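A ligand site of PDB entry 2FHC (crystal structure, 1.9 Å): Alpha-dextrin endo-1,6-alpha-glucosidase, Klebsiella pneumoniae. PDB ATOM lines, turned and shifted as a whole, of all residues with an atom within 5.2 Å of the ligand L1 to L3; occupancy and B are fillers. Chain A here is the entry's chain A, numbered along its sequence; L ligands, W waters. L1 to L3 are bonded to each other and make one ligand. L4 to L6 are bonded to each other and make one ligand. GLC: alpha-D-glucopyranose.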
ATOM      1  N   ALA A 641     -25.397   7.055   1.611  1.00  0.00           N
ATOM      2  CA  ALA A 641     -24.558   6.410   2.624  1.00  0.00           C
ATOM      3  C   ALA A 641     -23.124   6.172   2.152  1.00  0.00           C
ATOM      4  O   ALA A 641     -22.195   6.144   2.965  1.00  0.00           O
ATOM      5  CB  ALA A 641     -25.184   5.090   3.057  1.00  0.00           C
ATOM      6  N   THR A 642     -22.949   5.986   0.845  1.00  0.00           N
ATOM      7  CA  THR A 642     -21.627   5.749   0.273  1.00  0.00           C
ATOM      8  C   THR A 642     -20.789   7.024   0.295  1.00  0.00           C
ATOM      9  O   THR A 642     -19.550   6.950   0.342  1.00  0.00           O
ATOM     10  CB  THR A 642     -21.712   5.275  -1.196  1.00  0.00           C
ATOM     11  OG1 THR A 642     -22.340   6.284  -1.987  1.00  0.00           O
ATOM     12  CG2 THR A 642     -22.506   3.982  -1.306  1.00  0.00           C
ATOM     13  N   CYS A 643     -21.475   8.158   0.255  1.00  0.00           N
ATOM     14  CA  CYS A 643     -20.877   9.500   0.238  1.00  0.00           C
ATOM     15  C   CYS A 643     -21.649  10.351  -0.725  1.00  0.00           C
ATOM     16  O   CYS A 643     -21.863  11.550  -0.532  1.00  0.00           O
ATOM     17  CB  CYS A 643     -19.469   9.489  -0.349  1.00  0.00           C
ATOM     18  SG  CYS A 643     -19.317   8.925  -2.101  1.00  0.00           S
ATOM     19  N   LEU A 678     -16.175  -0.060  -1.636  1.00  0.00           N
ATOM     20  CA  LEU A 678     -17.389  -0.318  -0.863  1.00  0.00           C
ATOM     21  C   LEU A 678     -18.188  -1.521  -1.372  1.00  0.00           C
ATOM     22  O   LEU A 678     -19.399  -1.424  -1.629  1.00  0.00           O
ATOM     23  CB  LEU A 678     -18.271   0.929  -0.814  1.00  0.00           C
ATOM     24  CG  LEU A 678     -17.616   2.138  -0.125  1.00  0.00           C
ATOM     25  CD1 LEU A 678     -18.590   3.304  -0.118  1.00  0.00           C
ATOM     26  CD2 LEU A 678     -17.222   1.762   1.291  1.00  0.00           C
ATOM     27  N   GLU A 706     -13.597  -3.839  -0.149  1.00  0.00           N
ATOM     28  CA  GLU A 706     -13.939  -3.431   1.214  1.00  0.00           C
ATOM     29  C   GLU A 706     -15.191  -4.166   1.677  1.00  0.00           C
ATOM     30  O   GLU A 706     -16.283  -3.871   1.201  1.00  0.00           O
ATOM     31  CB  GLU A 706     -14.217  -1.926   1.281  1.00  0.00           C
ATOM     32  CG  GLU A 706     -13.091  -1.035   0.799  1.00  0.00           C
ATOM     33  CD  GLU A 706     -13.466   0.442   0.883  1.00  0.00           C
ATOM     34  OE1 GLU A 706     -13.376   1.037   1.990  1.00  0.00           O
ATOM     35  OE2 GLU A 706     -13.871   1.002  -0.151  1.00  0.00           O
ATOM     36  N   TRP A 708     -16.779  -4.120   4.731  1.00  0.00           N
ATOM     37  CA  TRP A 708     -17.195  -3.618   6.048  1.00  0.00           C
ATOM     38  C   TRP A 708     -18.710  -3.840   6.181  1.00  0.00           C
ATOM     39  O   TRP A 708     -19.293  -4.592   5.408  1.00  0.00           O
ATOM     40  CB  TRP A 708     -16.901  -2.125   6.168  1.00  0.00           C
ATOM     41  CG  TRP A 708     -15.569  -1.663   5.568  1.00  0.00           C
ATOM     42  CD1 TRP A 708     -15.399  -0.674   4.640  1.00  0.00           C
ATOM     43  CD2 TRP A 708     -14.252  -2.145   5.883  1.00  0.00           C
ATOM     44  NE1 TRP A 708     -14.059  -0.504   4.376  1.00  0.00           N
ATOM     45  CE2 TRP A 708     -13.338  -1.393   5.114  1.00  0.00           C
ATOM     46  CE3 TRP A 708     -13.754  -3.136   6.749  1.00  0.00           C
ATOM     47  CZ2 TRP A 708     -11.953  -1.599   5.181  1.00  0.00           C
ATOM     48  CZ3 TRP A 708     -12.382  -3.335   6.814  1.00  0.00           C
ATOM     49  CH2 TRP A 708     -11.485  -2.572   6.036  1.00  0.00           C
ATOM     50  N   ASP A 709     -19.340  -3.200   7.161  1.00  0.00           N
ATOM     51  CA  ASP A 709     -20.797  -3.345   7.327  1.00  0.00           C
ATOM     52  C   ASP A 709     -21.453  -2.138   6.651  1.00  0.00           C
ATOM     53  O   ASP A 709     -21.245  -0.992   7.054  1.00  0.00           O
ATOM     54  CB  ASP A 709     -21.193  -3.385   8.795  1.00  0.00           C
ATOM     55  CG  ASP A 709     -22.657  -3.798   8.996  1.00  0.00           C
ATOM     56  OD1 ASP A 709     -23.498  -3.398   8.170  1.00  0.00           O
ATOM     57  OD2 ASP A 709     -22.950  -4.514   9.970  1.00  0.00           O
ATOM     58  N   ASP A 734      -9.177  -5.346   8.752  1.00  0.00           N
ATOM     59  CA  ASP A 734      -8.876  -4.211   9.609  1.00  0.00           C
ATOM     60  C   ASP A 734      -8.293  -4.646  10.957  1.00  0.00           C
ATOM     61  O   ASP A 734      -7.965  -3.811  11.785  1.00  0.00           O
ATOM     62  CB  ASP A 734     -10.132  -3.333   9.817  1.00  0.00           C
ATOM     63  CG  ASP A 734     -11.412  -4.135  10.078  1.00  0.00           C
ATOM     64  OD1 ASP A 734     -11.407  -5.378   9.946  1.00  0.00           O
ATOM     65  OD2 ASP A 734     -12.442  -3.499  10.403  1.00  0.00           O
ATOM     66  N   ARG A 737      -4.237  -4.460  10.776  1.00  0.00           N
ATOM     67  CA  ARG A 737      -4.089  -3.043  10.436  1.00  0.00           C
ATOM     68  C   ARG A 737      -4.132  -2.151  11.686  1.00  0.00           C
ATOM     69  O   ARG A 737      -3.199  -1.406  11.974  1.00  0.00           O
ATOM     70  CB  ARG A 737      -5.211  -2.622   9.480  1.00  0.00           C
ATOM     71  CG  ARG A 737      -5.245  -1.139   9.130  1.00  0.00           C
ATOM     72  CD  ARG A 737      -6.606  -0.744   8.548  1.00  0.00           C
ATOM     73  NE  ARG A 737      -7.585  -0.435   9.589  1.00  0.00           N
ATOM     74  CZ  ARG A 737      -8.888  -0.284   9.377  1.00  0.00           C
ATOM     75  NH1 ARG A 737      -9.391  -0.423   8.152  1.00  0.00           N
ATOM     76  NH2 ARG A 737      -9.697   0.033  10.386  1.00  0.00           N
ATOM     77  N   ASP A 738      -5.236  -2.235  12.425  1.00  0.00           N
ATOM     78  CA  ASP A 738      -5.391  -1.416  13.637  1.00  0.00           C
ATOM     79  C   ASP A 738      -4.489  -1.847  14.796  1.00  0.00           C
ATOM     80  O   ASP A 738      -4.022  -1.006  15.570  1.00  0.00           O
ATOM     81  CB  ASP A 738      -6.862  -1.414  14.075  1.00  0.00           C
ATOM     82  CG  ASP A 738      -7.727  -0.551  13.188  1.00  0.00           C
ATOM     83  OD1 ASP A 738      -8.965  -0.602  13.341  1.00  0.00           O
ATOM     84  OD2 ASP A 738      -7.182   0.193  12.337  1.00  0.00           O
ATOM     85  N   PRO A 745      -9.501   4.478  12.441  1.00  0.00           N
ATOM     86  CA  PRO A 745      -9.661   5.584  11.490  1.00  0.00           C
ATOM     87  C   PRO A 745     -10.554   6.744  11.949  1.00  0.00           C
ATOM     88  O   PRO A 745     -10.512   7.816  11.350  1.00  0.00           O
ATOM     89  CB  PRO A 745     -10.213   4.892  10.242  1.00  0.00           C
ATOM     90  CG  PRO A 745     -10.968   3.728  10.788  1.00  0.00           C
ATOM     91  CD  PRO A 745     -10.053   3.228  11.887  1.00  0.00           C
ATOM     92  N   PHE A 746     -11.329   6.519  13.008  1.00  0.00           N
ATOM     93  CA  PHE A 746     -12.229   7.541  13.524  1.00  0.00           C
ATOM     94  C   PHE A 746     -11.666   8.395  14.662  1.00  0.00           C
ATOM     95  O   PHE A 746     -12.292   9.360  15.086  1.00  0.00           O
ATOM     96  CB  PHE A 746     -13.534   6.895  14.004  1.00  0.00           C
ATOM     97  CG  PHE A 746     -13.960   5.704  13.189  1.00  0.00           C
ATOM     98  CD1 PHE A 746     -13.319   4.469  13.341  1.00  0.00           C
ATOM     99  CD2 PHE A 746     -14.999   5.801  12.273  1.00  0.00           C
ATOM    100  CE1 PHE A 746     -13.713   3.358  12.591  1.00  0.00           C
ATOM    101  CE2 PHE A 746     -15.401   4.706  11.523  1.00  0.00           C
ATOM    102  CZ  PHE A 746     -14.756   3.479  11.678  1.00  0.00           C
ATOM    103  N   TYR A 812     -12.291  -8.457  18.257  1.00  0.00           N
ATOM    104  CA  TYR A 812     -11.869  -7.252  17.557  1.00  0.00           C
ATOM    105  C   TYR A 812     -13.042  -6.285  17.675  1.00  0.00           C
ATOM    106  O   TYR A 812     -14.008  -6.371  16.923  1.00  0.00           O
ATOM    107  CB  TYR A 812     -11.564  -7.518  16.076  1.00  0.00           C
ATOM    108  CG  TYR A 812     -11.291  -6.240  15.286  1.00  0.00           C
ATOM    109  CD1 TYR A 812     -10.194  -5.426  15.580  1.00  0.00           C
ATOM    110  CD2 TYR A 812     -12.151  -5.825  14.275  1.00  0.00           C
ATOM    111  CE1 TYR A 812      -9.951  -4.241  14.886  1.00  0.00           C
ATOM    112  CE2 TYR A 812     -11.925  -4.628  13.571  1.00  0.00           C
ATOM    113  CZ  TYR A 812     -10.823  -3.845  13.883  1.00  0.00           C
ATOM    114  OH  TYR A 812     -10.599  -2.677  13.203  1.00  0.00           O
ATOM    115  N   TYR A 829      -2.703  -5.034   5.662  1.00  0.00           N
ATOM    116  CA  TYR A 829      -2.091  -3.759   5.328  1.00  0.00           C
ATOM    117  C   TYR A 829      -1.957  -2.847   6.536  1.00  0.00           C
ATOM    118  O   TYR A 829      -2.672  -3.004   7.532  1.00  0.00           O
ATOM    119  CB  TYR A 829      -2.907  -3.033   4.232  1.00  0.00           C
ATOM    120  CG  TYR A 829      -4.286  -2.519   4.644  1.00  0.00           C
ATOM    121  CD1 TYR A 829      -5.323  -3.389   4.981  1.00  0.00           C
ATOM    122  CD2 TYR A 829      -4.563  -1.142   4.638  1.00  0.00           C
ATOM    123  CE1 TYR A 829      -6.589  -2.914   5.304  1.00  0.00           C
ATOM    124  CE2 TYR A 829      -5.838  -0.660   4.945  1.00  0.00           C
ATOM    125  CZ  TYR A 829      -6.847  -1.553   5.278  1.00  0.00           C
ATOM    126  OH  TYR A 829      -8.112  -1.077   5.549  1.00  0.00           O
ATOM    127  N   ASP A 834      -6.610   5.885   2.060  1.00  0.00           N
ATOM    128  CA  ASP A 834      -7.543   6.371   3.083  1.00  0.00           C
ATOM    129  C   ASP A 834      -6.868   6.539   4.442  1.00  0.00           C
ATOM    130  O   ASP A 834      -6.037   5.729   4.836  1.00  0.00           O
ATOM    131  CB  ASP A 834      -8.706   5.384   3.274  1.00  0.00           C
ATOM    132  CG  ASP A 834      -9.797   5.568   2.257  1.00  0.00           C
ATOM    133  OD1 ASP A 834     -10.461   4.558   1.931  1.00  0.00           O
ATOM    134  OD2 ASP A 834     -10.030   6.709   1.796  1.00  0.00           O
ATOM    135  N   ASN A 835      -7.257   7.585   5.157  1.00  0.00           N
ATOM    136  CA  ASN A 835      -6.729   7.865   6.486  1.00  0.00           C
ATOM    137  C   ASN A 835      -5.242   8.232   6.452  1.00  0.00           C
ATOM    138  O   ASN A 835      -4.624   8.260   5.389  1.00  0.00           O
ATOM    139  CB  ASN A 835      -6.983   6.659   7.395  1.00  0.00           C
ATOM    140  CG  ASN A 835      -8.461   6.276   7.428  1.00  0.00           C
ATOM    141  OD1 ASN A 835      -9.317   7.099   7.767  1.00  0.00           O
ATOM    142  ND2 ASN A 835      -8.760   5.032   7.076  1.00  0.00           N
ATOM    143  N   ARG A 889      -5.738  13.500   6.976  1.00  0.00           N
ATOM    144  CA  ARG A 889      -6.403  12.203   7.110  1.00  0.00           C
ATOM    145  C   ARG A 889      -7.089  11.722   5.828  1.00  0.00           C
ATOM    146  O   ARG A 889      -6.957  10.570   5.439  1.00  0.00           O
ATOM    147  CB  ARG A 889      -7.442  12.218   8.242  1.00  0.00           C
ATOM    148  CG  ARG A 889      -8.144  10.859   8.415  1.00  0.00           C
ATOM    149  CD  ARG A 889      -9.329  10.919   9.388  1.00  0.00           C
ATOM    150  NE  ARG A 889     -10.464  11.649   8.819  1.00  0.00           N
ATOM    151  CZ  ARG A 889     -11.269  11.177   7.871  1.00  0.00           C
ATOM    152  NH1 ARG A 889     -11.074   9.958   7.368  1.00  0.00           N
ATOM    153  NH2 ARG A 889     -12.259  11.923   7.406  1.00  0.00           N
ATOM    154  N   ASP A 890      -7.838  12.619   5.188  1.00  0.00           N
ATOM    155  CA  ASP A 890      -8.584  12.288   3.961  1.00  0.00           C
ATOM    156  C   ASP A 890      -8.152  13.250   2.847  1.00  0.00           C
ATOM    157  O   ASP A 890      -8.785  14.281   2.640  1.00  0.00           O
ATOM    158  CB  ASP A 890     -10.081  12.433   4.262  1.00  0.00           C
ATOM    159  CG  ASP A 890     -10.963  11.945   3.131  1.00  0.00           C
ATOM    160  OD1 ASP A 890     -12.185  12.128   3.239  1.00  0.00           O
ATOM    161  OD2 ASP A 890     -10.433  11.389   2.141  1.00  0.00           O
HETATM  162  C1  GLC L   1     -14.932  -0.472  10.109  1.00  0.00           C
HETATM  163  C2  GLC L   1     -13.508  -0.520   9.505  1.00  0.00           C
HETATM  164  C3  GLC L   1     -13.130   0.828   8.899  1.00  0.00           C
HETATM  165  C4  GLC L   1     -14.195   1.250   7.884  1.00  0.00           C
HETATM  166  C5  GLC L   1     -15.551   1.305   8.593  1.00  0.00           C
HETATM  167  C6  GLC L   1     -16.681   1.702   7.654  1.00  0.00           C
HETATM  168  O1  GLC L   1     -14.957   0.391  11.189  1.00  0.00           O
HETATM  169  O2  GLC L   1     -12.570  -0.860  10.525  1.00  0.00           O
HETATM  170  O3  GLC L   1     -11.868   0.733   8.248  1.00  0.00           O
HETATM  171  O4  GLC L   1     -13.846   2.541   7.328  1.00  0.00           O
HETATM  172  O5  GLC L   1     -15.872  -0.003   9.123  1.00  0.00           O
HETATM  173  O6  GLC L   1     -17.931   1.671   8.331  1.00  0.00           O
HETATM  174  C1  GLC L   2     -13.374   2.492   6.011  1.00  0.00           C
HETATM  175  C2  GLC L   2     -12.126   3.373   5.851  1.00  0.00           C
HETATM  176  C3  GLC L   2     -12.517   4.850   5.879  1.00  0.00           C
HETATM  177  C4  GLC L   2     -13.579   5.124   4.817  1.00  0.00           C
HETATM  178  C5  GLC L   2     -14.788   4.222   5.071  1.00  0.00           C
HETATM  179  C6  GLC L   2     -15.854   4.375   3.996  1.00  0.00           C
HETATM  180  O2  GLC L   2     -11.188   3.098   6.882  1.00  0.00           O
HETATM  181  O3  GLC L   2     -11.378   5.666   5.645  1.00  0.00           O
HETATM  182  O4  GLC L   2     -13.974   6.512   4.888  1.00  0.00           O
HETATM  183  O5  GLC L   2     -14.385   2.836   5.061  1.00  0.00           O
HETATM  184  O6  GLC L   2     -16.668   5.507   4.264  1.00  0.00           O
HETATM  185  C1  GLC L   3     -13.646   7.265   3.759  1.00  0.00           C
HETATM  186  C2  GLC L   3     -13.111   8.636   4.196  1.00  0.00           C
HETATM  187  C3  GLC L   3     -14.223   9.425   4.888  1.00  0.00           C
HETATM  188  C4  GLC L   3     -15.442   9.541   3.961  1.00  0.00           C
HETATM  189  C5  GLC L   3     -15.878   8.148   3.478  1.00  0.00           C
HETATM  190  C6  GLC L   3     -16.973   8.192   2.437  1.00  0.00           C
HETATM  191  O2  GLC L   3     -12.016   8.466   5.076  1.00  0.00           O
HETATM  192  O3  GLC L   3     -13.746  10.727   5.218  1.00  0.00           O
HETATM  193  O4  GLC L   3     -16.507  10.158   4.658  1.00  0.00           O
HETATM  194  O5  GLC L   3     -14.765   7.442   2.896  1.00  0.00           O
HETATM  195  O6  GLC L   3     -17.470   6.883   2.166  1.00  0.00           O
HETATM  196  C1  GLC L   4     -13.958   3.915  -0.261  1.00  0.00           C
HETATM  197  C2  GLC L   4     -12.671   4.635  -0.689  1.00  0.00           C
HETATM  198  C3  GLC L   4     -12.716   6.073  -0.165  1.00  0.00           C
HETATM  199  C4  GLC L   4     -13.924   6.772  -0.785  1.00  0.00           C
HETATM  200  C5  GLC L   4     -15.221   5.984  -0.467  1.00  0.00           C
HETATM  201  C6  GLC L   4     -16.377   6.520  -1.286  1.00  0.00           C
HETATM  202  O1  GLC L   4     -14.087   3.933   1.118  1.00  0.00           O
HETATM  203  O2  GLC L   4     -11.533   3.956  -0.185  1.00  0.00           O
HETATM  204  O3  GLC L   4     -11.513   6.751  -0.502  1.00  0.00           O
HETATM  205  O4  GLC L   4     -14.046   8.115  -0.281  1.00  0.00           O
HETATM  206  O5  GLC L   4     -15.096   4.577  -0.827  1.00  0.00           O
HETATM  207  O6  GLC L   4     -16.228   6.158  -2.651  1.00  0.00           O
HETATM  208  C1  GLC L   5     -13.402   9.120  -1.006  1.00  0.00           C
HETATM  209  C2  GLC L   5     -13.048  10.301  -0.077  1.00  0.00           C
HETATM  210  C3  GLC L   5     -14.312  11.063   0.316  1.00  0.00           C
HETATM  211  C4  GLC L   5     -15.069  11.511  -0.945  1.00  0.00           C
HETATM  212  C5  GLC L   5     -15.394  10.271  -1.796  1.00  0.00           C
HETATM  213  C6  GLC L   5     -16.103  10.615  -3.094  1.00  0.00           C
HETATM  214  O2  GLC L   5     -12.394   9.826   1.090  1.00  0.00           O
HETATM  215  O3  GLC L   5     -13.970  12.210   1.105  1.00  0.00           O
HETATM  216  O4  GLC L   5     -16.288  12.173  -0.558  1.00  0.00           O
HETATM  217  O5  GLC L   5     -14.167   9.578  -2.128  1.00  0.00           O
HETATM  218  O6  GLC L   5     -15.316  11.464  -3.913  1.00  0.00           O
HETATM  219  C1  GLC L   6     -16.222  13.579  -0.558  1.00  0.00           C
HETATM  220  C2  GLC L   6     -16.993  14.134   0.639  1.00  0.00           C
HETATM  221  C3  GLC L   6     -18.485  13.850   0.465  1.00  0.00           C
HETATM  222  C4  GLC L   6     -18.966  14.439  -0.870  1.00  0.00           C
HETATM  223  C5  GLC L   6     -18.111  13.889  -2.024  1.00  0.00           C
HETATM  224  C6  GLC L   6     -18.453  14.527  -3.362  1.00  0.00           C
HETATM  225  O2  GLC L   6     -16.517  13.542   1.832  1.00  0.00           O
HETATM  226  O3  GLC L   6     -19.203  14.426   1.539  1.00  0.00           O
HETATM  227  O4  GLC L   6     -20.338  14.098  -1.084  1.00  0.00           O
HETATM  228  O5  GLC L   6     -16.711  14.139  -1.775  1.00  0.00           O
HETATM  229  O6  GLC L   6     -18.347  15.934  -3.308  1.00  0.00           O
HETATM  230  O   HOH W   1     -19.292   5.558   3.581  1.00  0.00           O
HETATM  231  O   HOH W   2     -12.685  -0.054  13.062  1.00  0.00           O
HETATM  232  O   HOH W   3     -18.555  -1.180   9.261  1.00  0.00           O
HETATM  233  O   HOH W   4     -20.164   1.376   6.756  1.00  0.00           O
HETATM  234  O   HOH W   5     -17.118  -0.090  12.686  1.00  0.00           O
HETATM  235  O   HOH W   6      -9.719   8.790   3.579  1.00  0.00           O
HETATM  236  O   HOH W   7      -9.144   1.439   5.031  1.00  0.00           O
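O2 of GLC L5 is in hydrogen-bond range of OD2 of Asp 890, at 2.7 Å. The side-chain carboxylate (OD1) of Asp 834 lies within hydrogen-bond range of an oxygen (O2) of GLC L4, 2.4 Å away. An oxygen (O2) of GLC L1 is in hydrogen-bond range of the side-chain carboxylate (OD2) of Asp 734. An oxygen (O4) of GLC L6 is in hydrogen-bond range of the backbone carbonyl oxygen of Cys 643, 3.0 Å away. An oxygen (O6) of GLC L3 is in hydrogen-bond range of the backbone carbonyl oxygen of Thr 642. O1 of GLC L4 sits at hydrogen-bond distance from OE1 of Glu 706, 3.1 Å away. O5 of GLC L2 is in hydrogen-bond range of NE1 of Trp 708 (3.4 Å). The guanidinium group (NH1) of Arg 889 sits at hydrogen-bond distance from an oxygen (O2) of GLC L3, at 2.9 Å. The side-chain amide nitrogen (ND2) of Asn 835 is in hydrogen-bond range of an oxygen (O3) of GLC L2, 3.1 Å away. The side-chain carboxylate of Asp 890 is in hydrogen-bond range of an oxygen (O3) of GLC L3 (2.9 Å). The guanidinium group (NH1) of Arg 737 sits at hydrogen-bond distance from an oxygen (O3) of GLC L1 (2.7 Å).
The indole nitrogen (NE1) of Trp 708 lies within hydrogen-bond range of the side-chain carboxylate (OE1) of Glu 706 (2.9 Å). The backbone carbonyl oxygen of Asp 734 is in hydrogen-bond range of the side-chain hydroxyl of Tyr 812 (3.2 Å). The side-chain hydroxyl (OH) of Tyr 812 lies within hydrogen-bond range of the side-chain carboxylate (OD1) of Asp 738. OE2 of Glu 706 sits at hydrogen-bond distance from N of Leu 678 (2.9 Å). The backbone NH of Asn 835 lies close to the backbone carbonyl oxygen of Arg 889 (3.0 Å). The side-chain hydroxyl (OH) of Tyr 829 sits at hydrogen-bond distance from the guanidinium group (NH1) of Arg 737, 3.0 Å away. OD2 of Asp 738 lies within salt-bridge range of NE of Arg 737.
Merely in contact with the ligand L1 to L3: Cys 643, Glu 706, Pro 745, Phe 746, Tyr 812 and Asp 834. Hydrophobic or aromatic side chains within 4 Å of the ligand L1 to L3: Trp 708, Pro 745 and Phe 746. 13 residues have an atom within 4 Å of the ligand L1 to L3: Thr 642, Cys 643, Glu 706, Trp 708, Asp 734, Arg 737, Pro 745, Phe 746, Tyr 812, Asp 834, Asn 835, Arg 889 and Asp 890. The nearest printed residue that does not touch the ligand L1 to L3 is Leu 678 (4.002 Å).
Water W1 bridges O6 of GLC L3 (2.7 Å) and O of Ala 641 (3.0 Å). Water W2 bridges an oxygen (O2) of GLC L1 (2.7 Å) and the side-chain hydroxyl of Tyr 812 (3.4 Å). Water W4 bridges O of Asp 709 (2.6 Å) and O6 of GLC L1 (2.7 Å). Water W6 lies within hydrogen-bond range of the side-chain carboxylate (OD2) of Asp 834 (2.8 Å), an oxygen (O2) of GLC L3 (2.8 Å), the side-chain carboxylate (OD2) of Asp 890 (3.1 Å) and the backbone NH (N) of Asn 835 (3.2 Å). Water W3 bridges O5 of GLC L1 (2.9 Å) and N of Asp 709 (3.0 Å). Water W7 lies within hydrogen-bond range of the side-chain hydroxyl of Tyr 829 (2.8 Å) and an oxygen (O2) of GLC L2 (3.2 Å).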
